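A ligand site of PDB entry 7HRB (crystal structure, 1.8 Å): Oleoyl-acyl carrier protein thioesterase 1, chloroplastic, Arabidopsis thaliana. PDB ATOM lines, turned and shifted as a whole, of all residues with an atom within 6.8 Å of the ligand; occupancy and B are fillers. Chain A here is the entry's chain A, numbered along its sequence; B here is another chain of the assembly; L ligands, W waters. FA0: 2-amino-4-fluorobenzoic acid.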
ATOM      1  N   ALA A  28      21.191  24.298 -21.550  1.00  0.00           N
ATOM      2  CA  ALA A  28      19.801  24.386 -21.958  1.00  0.00           C
ATOM      3  C   ALA A  28      18.856  24.488 -20.755  1.00  0.00           C
ATOM      4  O   ALA A  28      19.060  23.829 -19.752  1.00  0.00           O
ATOM      5  CB  ALA A  28      19.425  23.166 -22.809  1.00  0.00           C
ATOM      6  N   THR A  29      17.856  25.360 -20.849  1.00  0.00           N
ATOM      7  CA  THR A  29      16.838  25.474 -19.818  1.00  0.00           C
ATOM      8  C   THR A  29      15.850  24.287 -19.982  1.00  0.00           C
ATOM      9  O   THR A  29      15.801  23.655 -21.054  1.00  0.00           O
ATOM     10  CB  THR A  29      16.042  26.784 -20.032  1.00  0.00           C
ATOM     11  OG1 THR A  29      15.402  26.785 -21.313  1.00  0.00           O
ATOM     12  CG2 THR A  29      16.883  28.032 -19.800  1.00  0.00           C
ATOM     13  N   VAL A  30      15.080  23.966 -18.942  1.00  0.00           N
ATOM     14  CA  VAL A  30      14.074  22.921 -19.025  1.00  0.00           C
ATOM     15  C   VAL A  30      12.948  23.315 -20.003  1.00  0.00           C
ATOM     16  O   VAL A  30      12.340  22.421 -20.581  1.00  0.00           O
ATOM     17  CB  VAL A  30      13.553  22.430 -17.655  1.00  0.00           C
ATOM     18  CG1 VAL A  30      12.498  23.389 -17.084  1.00  0.00           C
ATOM     19  CG2 VAL A  30      13.001  21.012 -17.759  1.00  0.00           C
ATOM     20  N   GLU A  31      12.713  24.629 -20.236  1.00  0.00           N
ATOM     21  CA  GLU A  31      11.700  25.037 -21.200  1.00  0.00           C
ATOM     22  C   GLU A  31      12.212  24.745 -22.613  1.00  0.00           C
ATOM     23  O   GLU A  31      11.445  24.302 -23.445  1.00  0.00           O
ATOM     24  CB  GLU A  31      11.330  26.516 -21.019  1.00  0.00           C
ATOM     25  CG  GLU A  31      10.496  26.787 -19.789  1.00  0.00           C
ATOM     26  CD  GLU A  31      10.045  28.228 -19.744  1.00  0.00           C
ATOM     27  OE1 GLU A  31      10.662  29.030 -19.006  1.00  0.00           O
ATOM     28  OE2 GLU A  31       9.059  28.557 -20.432  1.00  0.00           O
ATOM     29  N   THR A  32      13.534  24.913 -22.870  1.00  0.00           N
ATOM     30  CA  THR A  32      14.119  24.531 -24.161  1.00  0.00           C
ATOM     31  C   THR A  32      13.968  23.013 -24.335  1.00  0.00           C
ATOM     32  O   THR A  32      13.514  22.579 -25.399  1.00  0.00           O
ATOM     33  CB  THR A  32      15.617  24.894 -24.223  1.00  0.00           C
ATOM     34  OG1 THR A  32      15.708  26.298 -24.402  1.00  0.00           O
ATOM     35  CG2 THR A  32      16.346  24.190 -25.382  1.00  0.00           C
ATOM     36  N   TYR A  80      22.096  18.788 -18.201  1.00  0.00           N
ATOM     37  CA  TYR A  80      21.556  19.656 -19.239  1.00  0.00           C
ATOM     38  C   TYR A  80      22.636  19.864 -20.287  1.00  0.00           C
ATOM     39  O   TYR A  80      23.767  20.184 -19.939  1.00  0.00           O
ATOM     40  CB  TYR A  80      21.130  21.007 -18.649  1.00  0.00           C
ATOM     41  CG  TYR A  80      19.912  20.947 -17.773  1.00  0.00           C
ATOM     42  CD1 TYR A  80      18.643  21.072 -18.307  1.00  0.00           C
ATOM     43  CD2 TYR A  80      20.021  20.771 -16.390  1.00  0.00           C
ATOM     44  CE1 TYR A  80      17.512  21.070 -17.502  1.00  0.00           C
ATOM     45  CE2 TYR A  80      18.893  20.720 -15.584  1.00  0.00           C
ATOM     46  CZ  TYR A  80      17.640  20.886 -16.142  1.00  0.00           C
ATOM     47  OH  TYR A  80      16.523  20.864 -15.342  1.00  0.00           O
ATOM     48  N   ILE A 200       5.072  25.630 -17.914  1.00  0.00           N
ATOM     49  CA  ILE A 200       6.262  25.217 -17.192  1.00  0.00           C
ATOM     50  C   ILE A 200       7.017  26.485 -16.734  1.00  0.00           C
ATOM     51  O   ILE A 200       7.418  26.593 -15.572  1.00  0.00           O
ATOM     52  CB  ILE A 200       7.157  24.274 -18.069  1.00  0.00           C
ATOM     53  CG1 ILE A 200       6.456  22.945 -18.346  1.00  0.00           C
ATOM     54  CG2 ILE A 200       8.512  24.062 -17.417  1.00  0.00           C
ATOM     55  CD1 ILE A 200       7.192  22.010 -19.353  1.00  0.00           C
ATOM     56  N   GLY A 201       7.166  27.462 -17.633  1.00  0.00           N
ATOM     57  CA  GLY A 201       7.796  28.745 -17.294  1.00  0.00           C
ATOM     58  C   GLY A 201       7.083  29.488 -16.182  1.00  0.00           C
ATOM     59  O   GLY A 201       7.707  29.947 -15.212  1.00  0.00           O
ATOM     60  N   TRP A 202       5.747  29.541 -16.264  1.00  0.00           N
ATOM     61  CA  TRP A 202       4.909  30.189 -15.249  1.00  0.00           C
ATOM     62  C   TRP A 202       5.005  29.518 -13.862  1.00  0.00           C
ATOM     63  O   TRP A 202       5.072  30.226 -12.855  1.00  0.00           O
ATOM     64  CB  TRP A 202       3.452  30.300 -15.724  1.00  0.00           C
ATOM     65  CG  TRP A 202       3.193  31.285 -16.814  1.00  0.00           C
ATOM     66  CD1 TRP A 202       3.946  32.382 -17.138  1.00  0.00           C
ATOM     67  CD2 TRP A 202       2.028  31.330 -17.661  1.00  0.00           C
ATOM     68  NE1 TRP A 202       3.355  33.068 -18.163  1.00  0.00           N
ATOM     69  CE2 TRP A 202       2.173  32.456 -18.498  1.00  0.00           C
ATOM     70  CE3 TRP A 202       0.904  30.506 -17.821  1.00  0.00           C
ATOM     71  CZ2 TRP A 202       1.215  32.784 -19.478  1.00  0.00           C
ATOM     72  CZ3 TRP A 202      -0.028  30.818 -18.810  1.00  0.00           C
ATOM     73  CH2 TRP A 202       0.130  31.950 -19.607  1.00  0.00           C
ATOM     74  N   LEU A 204       7.671  27.874 -12.701  1.00  0.00           N
ATOM     75  CA  LEU A 204       9.016  28.158 -12.233  1.00  0.00           C
ATOM     76  C   LEU A 204       9.260  29.634 -11.863  1.00  0.00           C
ATOM     77  O   LEU A 204      10.199  29.917 -11.147  1.00  0.00           O
ATOM     78  CB  LEU A 204      10.034  27.640 -13.263  1.00  0.00           C
ATOM     79  CG  LEU A 204      10.006  26.109 -13.524  1.00  0.00           C
ATOM     80  CD1 LEU A 204      10.765  25.731 -14.776  1.00  0.00           C
ATOM     81  CD2 LEU A 204      10.534  25.312 -12.315  1.00  0.00           C
ATOM     82  N   GLU A 205       8.387  30.540 -12.311  1.00  0.00           N
ATOM     83  CA  GLU A 205       8.492  31.963 -11.976  1.00  0.00           C
ATOM     84  C   GLU A 205       8.371  32.207 -10.450  1.00  0.00           C
ATOM     85  O   GLU A 205       8.879  33.204  -9.949  1.00  0.00           O
ATOM     86  CB  GLU A 205       7.396  32.777 -12.683  1.00  0.00           C
ATOM     87  CG  GLU A 205       7.764  33.343 -14.047  1.00  0.00           C
ATOM     88  CD  GLU A 205       9.049  34.146 -14.106  1.00  0.00           C
ATOM     89  OE1 GLU A 205      10.097  33.571 -14.472  1.00  0.00           O
ATOM     90  OE2 GLU A 205       9.009  35.368 -13.854  1.00  0.00           O
ATOM     91  N   SER A 206       7.638  31.337  -9.732  1.00  0.00           N
ATOM     92  CA  SER A 206       7.459  31.546  -8.302  1.00  0.00           C
ATOM     93  C   SER A 206       8.577  30.919  -7.432  1.00  0.00           C
ATOM     94  O   SER A 206       8.499  31.036  -6.217  1.00  0.00           O
ATOM     95  CB  SER A 206       6.065  31.108  -7.846  1.00  0.00           C
ATOM     96  OG  SER A 206       5.751  29.811  -8.292  1.00  0.00           O
ATOM     97  N   ILE A 207       9.578  30.260  -8.031  1.00  0.00           N
ATOM     98  CA  ILE A 207      10.708  29.695  -7.275  1.00  0.00           C
ATOM     99  C   ILE A 207      11.602  30.853  -6.849  1.00  0.00           C
ATOM    100  O   ILE A 207      11.892  31.721  -7.676  1.00  0.00           O
ATOM    101  CB  ILE A 207      11.529  28.699  -8.144  1.00  0.00           C
ATOM    102  CG1 ILE A 207      10.711  27.459  -8.533  1.00  0.00           C
ATOM    103  CG2 ILE A 207      12.872  28.320  -7.472  1.00  0.00           C
ATOM    104  CD1 ILE A 207      10.296  26.644  -7.351  1.00  0.00           C
ATOM    105  N   PRO A 208      12.042  30.946  -5.584  1.00  0.00           N
ATOM    106  CA  PRO A 208      12.914  32.077  -5.196  1.00  0.00           C
ATOM    107  C   PRO A 208      14.268  32.070  -5.953  1.00  0.00           C
ATOM    108  O   PRO A 208      14.788  31.003  -6.273  1.00  0.00           O
ATOM    109  CB  PRO A 208      13.077  31.925  -3.677  1.00  0.00           C
ATOM    110  CG  PRO A 208      12.649  30.560  -3.343  1.00  0.00           C
ATOM    111  CD  PRO A 208      11.768  30.028  -4.460  1.00  0.00           C
ATOM    112  N   GLN A 209      14.789  33.261  -6.252  1.00  0.00           N
ATOM    113  CA  GLN A 209      16.058  33.448  -6.964  1.00  0.00           C
ATOM    114  C   GLN A 209      17.243  32.751  -6.290  1.00  0.00           C
ATOM    115  O   GLN A 209      18.090  32.196  -7.000  1.00  0.00           O
ATOM    116  CB  GLN A 209      16.365  34.935  -7.151  1.00  0.00           C
ATOM    117  CG  GLN A 209      17.500  35.226  -8.128  1.00  0.00           C
ATOM    118  CD  GLN A 209      17.114  34.784  -9.512  1.00  0.00           C
ATOM    119  OE1 GLN A 209      16.005  35.041  -9.988  1.00  0.00           O
ATOM    120  NE2 GLN A 209      18.022  34.109 -10.197  1.00  0.00           N
ATOM    121  N   VAL A 212      17.235  29.209  -7.483  1.00  0.00           N
ATOM    122  CA  VAL A 212      17.643  29.170  -8.889  1.00  0.00           C
ATOM    123  C   VAL A 212      19.164  29.350  -9.058  1.00  0.00           C
ATOM    124  O   VAL A 212      19.803  28.624  -9.819  1.00  0.00           O
ATOM    125  CB  VAL A 212      16.851  30.240  -9.690  1.00  0.00           C
ATOM    126  CG1 VAL A 212      17.361  30.351 -11.127  1.00  0.00           C
ATOM    127  CG2 VAL A 212      15.363  29.929  -9.657  1.00  0.00           C
ATOM    128  N   HIS A 215      20.894  25.939  -7.087  1.00  0.00           N
ATOM    129  CA  HIS A 215      20.396  24.579  -7.325  1.00  0.00           C
ATOM    130  C   HIS A 215      20.082  24.350  -8.799  1.00  0.00           C
ATOM    131  O   HIS A 215      19.793  25.301  -9.533  1.00  0.00           O
ATOM    132  CB  HIS A 215      19.088  24.320  -6.533  1.00  0.00           C
ATOM    133  CG  HIS A 215      19.240  24.223  -5.051  1.00  0.00           C
ATOM    134  ND1 HIS A 215      19.712  25.284  -4.301  1.00  0.00           N
ATOM    135  CD2 HIS A 215      18.930  23.195  -4.218  1.00  0.00           C
ATOM    136  CE1 HIS A 215      19.697  24.878  -3.037  1.00  0.00           C
ATOM    137  NE2 HIS A 215      19.233  23.622  -2.935  1.00  0.00           N
ATOM    138  N   LEU A 217      17.407  22.130 -11.364  1.00  0.00           N
ATOM    139  CA  LEU A 217      16.135  21.418 -11.412  1.00  0.00           C
ATOM    140  C   LEU A 217      16.393  19.993 -11.904  1.00  0.00           C
ATOM    141  O   LEU A 217      16.971  19.830 -12.975  1.00  0.00           O
ATOM    142  CB  LEU A 217      15.175  22.147 -12.357  1.00  0.00           C
ATOM    143  CG  LEU A 217      13.813  21.455 -12.532  1.00  0.00           C
ATOM    144  CD1 LEU A 217      13.027  21.522 -11.242  1.00  0.00           C
ATOM    145  CD2 LEU A 217      13.026  22.112 -13.672  1.00  0.00           C
ATOM    146  N   TRP A 283      14.846  19.856  -6.696  1.00  0.00           N
ATOM    147  CA  TRP A 283      16.070  20.595  -7.006  1.00  0.00           C
ATOM    148  C   TRP A 283      17.265  20.029  -6.230  1.00  0.00           C
ATOM    149  O   TRP A 283      17.140  19.651  -5.072  1.00  0.00           O
ATOM    150  CB  TRP A 283      15.904  22.096  -6.676  1.00  0.00           C
ATOM    151  CG  TRP A 283      14.758  22.756  -7.385  1.00  0.00           C
ATOM    152  CD1 TRP A 283      13.433  22.553  -7.167  1.00  0.00           C
ATOM    153  CD2 TRP A 283      14.845  23.716  -8.456  1.00  0.00           C
ATOM    154  NE1 TRP A 283      12.686  23.329  -8.021  1.00  0.00           N
ATOM    155  CE2 TRP A 283      13.527  24.066  -8.809  1.00  0.00           C
ATOM    156  CE3 TRP A 283      15.918  24.355  -9.094  1.00  0.00           C
ATOM    157  CZ2 TRP A 283      13.248  24.996  -9.820  1.00  0.00           C
ATOM    158  CZ3 TRP A 283      15.638  25.256 -10.113  1.00  0.00           C
ATOM    159  CH2 TRP A 283      14.313  25.561 -10.464  1.00  0.00           C
ATOM    160  N   ARG B 184       9.789  37.282 -18.000  1.00  0.00           N
ATOM    161  CA  ARG B 184       9.887  36.089 -17.158  1.00  0.00           C
ATOM    162  C   ARG B 184      11.317  35.524 -17.360  1.00  0.00           C
ATOM    163  O   ARG B 184      12.051  36.047 -18.186  1.00  0.00           O
ATOM    164  CB  ARG B 184       8.735  35.088 -17.404  1.00  0.00           C
ATOM    165  CG  ARG B 184       8.517  34.612 -18.841  1.00  0.00           C
ATOM    166  CD  ARG B 184       7.292  33.692 -18.918  1.00  0.00           C
ATOM    167  NE  ARG B 184       7.018  33.207 -20.281  1.00  0.00           N
ATOM    168  CZ  ARG B 184       7.457  32.048 -20.766  1.00  0.00           C
ATOM    169  NH1 ARG B 184       8.212  31.241 -20.023  1.00  0.00           N
ATOM    170  NH2 ARG B 184       7.134  31.680 -22.006  1.00  0.00           N
ATOM    171  N   ARG B 185      11.740  34.502 -16.596  1.00  0.00           N
ATOM    172  CA  ARG B 185      13.100  33.948 -16.742  1.00  0.00           C
ATOM    173  C   ARG B 185      13.459  33.517 -18.200  1.00  0.00           C
ATOM    174  O   ARG B 185      14.598  33.689 -18.591  1.00  0.00           O
ATOM    175  CB  ARG B 185      13.369  32.830 -15.724  1.00  0.00           C
ATOM    176  CG  ARG B 185      13.647  33.435 -14.343  1.00  0.00           C
ATOM    177  CD  ARG B 185      13.455  32.449 -13.179  1.00  0.00           C
ATOM    178  NE  ARG B 185      13.779  33.064 -11.894  1.00  0.00           N
ATOM    179  CZ  ARG B 185      13.162  32.799 -10.744  1.00  0.00           C
ATOM    180  NH1 ARG B 185      12.174  31.906 -10.703  1.00  0.00           N
ATOM    181  NH2 ARG B 185      13.522  33.430  -9.635  1.00  0.00           N
ATOM    182  N   ALA B 186      12.478  33.048 -19.007  1.00  0.00           N
ATOM    183  CA  ALA B 186      12.758  32.685 -20.403  1.00  0.00           C
ATOM    184  C   ALA B 186      13.139  33.894 -21.276  1.00  0.00           C
ATOM    185  O   ALA B 186      13.725  33.724 -22.333  1.00  0.00           O
ATOM    186  CB  ALA B 186      11.575  31.973 -21.030  1.00  0.00           C
HETATM  187  OAA FA0 L   1      15.228  25.905 -16.890  1.00  0.00           O
HETATM  188  CAB FA0 L   1      14.303  26.747 -16.882  1.00  0.00           C
HETATM  189  OAC FA0 L   1      13.524  26.928 -17.848  1.00  0.00           O
HETATM  190  CAD FA0 L   1      14.099  27.523 -15.610  1.00  0.00           C
HETATM  191  CAE FA0 L   1      14.949  27.217 -14.539  1.00  0.00           C
HETATM  192  CAF FA0 L   1      14.817  27.851 -13.314  1.00  0.00           C
HETATM  193  CAG FA0 L   1      13.834  28.786 -13.169  1.00  0.00           C
HETATM  194  FAH FA0 L   1      13.708  29.407 -11.961  1.00  0.00           F
HETATM  195  CAI FA0 L   1      12.980  29.162 -14.185  1.00  0.00           C
HETATM  196  CAJ FA0 L   1      13.088  28.494 -15.421  1.00  0.00           C
HETATM  197  NAK FA0 L   1      12.223  28.842 -16.431  1.00  0.00           N
HETATM  198  O   HOH W   1      13.548  29.324 -19.412  1.00  0.00           O
HETATM  199  O   HOH W   2      10.196  30.994 -15.313  1.00  0.00           O
HETATM  200  O   HOH W   3      16.575  24.321 -15.602  1.00  0.00           O
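An oxygen (OAA) of the ligand lies within hydrogen-bond range of the backbone NH (N) of Val 30 (2.8 Å).
An oxygen (OAC) of the ligand sits at hydrogen-bond distance from the backbone NH (N) of Glu 31, at 3.4 Å.
A nitrogen (NAK) of the ligand lies within hydrogen-bond range of the side-chain carboxylate (OE1) of Glu 31 (3.0 Å).
The side-chain carboxylate (OE2) of Glu 31 lies within salt-bridge range of the guanidinium group (NH1) of Arg 184 of chain B.
The guanidinium group (NH1) of Arg 185 of chain B is in hydrogen-bond range of the backbone carbonyl oxygen (O) of Leu 204, 2.8 Å away.
The backbone carbonyl oxygen of Ile 207 lies within hydrogen-bond range of the guanidinium group of Arg 185 of chain B (3.0 Å).
The backbone NH of Arg 185 of chain B sits at hydrogen-bond distance from the side-chain carboxylate of Glu 205.
NH2 of Arg 185 of chain B lies within hydrogen-bond range of OE1 of Gln 209 (3.0 Å).
The backbone NH of Thr 32 sits at hydrogen-bond distance from the side-chain hydroxyl of Thr 29 (3.1 Å).
Water W3 bridges an oxygen (OAA) of the ligand and the side-chain hydroxyl of Tyr 80.
Water W1 lies within hydrogen-bond range of an oxygen (OAC) of the ligand (2.9 Å) and the side-chain carboxylate of Glu 31 (2.9 Å).
Water W2 lies within hydrogen-bond range of O of Gly 201 (2.7 Å), OE1 of Glu 205 (2.7 Å) and NAK of the ligand (3.2 Å).
NH1 of Arg 185 of chain B lies close to FAH of the ligand, 3.2 Å away.
Merely in contact with the ligand: Val 212 (2.9 Å), Thr 29 (3.3 Å), Leu 204 (3.4 Å) and Trp 283 (3.7 Å).
Hydrophobic or aromatic side chains within 4 Å of the ligand: Val 30, Leu 204, Val 212 and Trp 283.
Within 4 Å of the ligand: Thr 29, Val 30, Glu 31, Leu 204, Val 212, Trp 283 and Arg 185 of chain B.
The nearest printed residue that does not touch the ligand is Ile 207 (4.5 Å).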
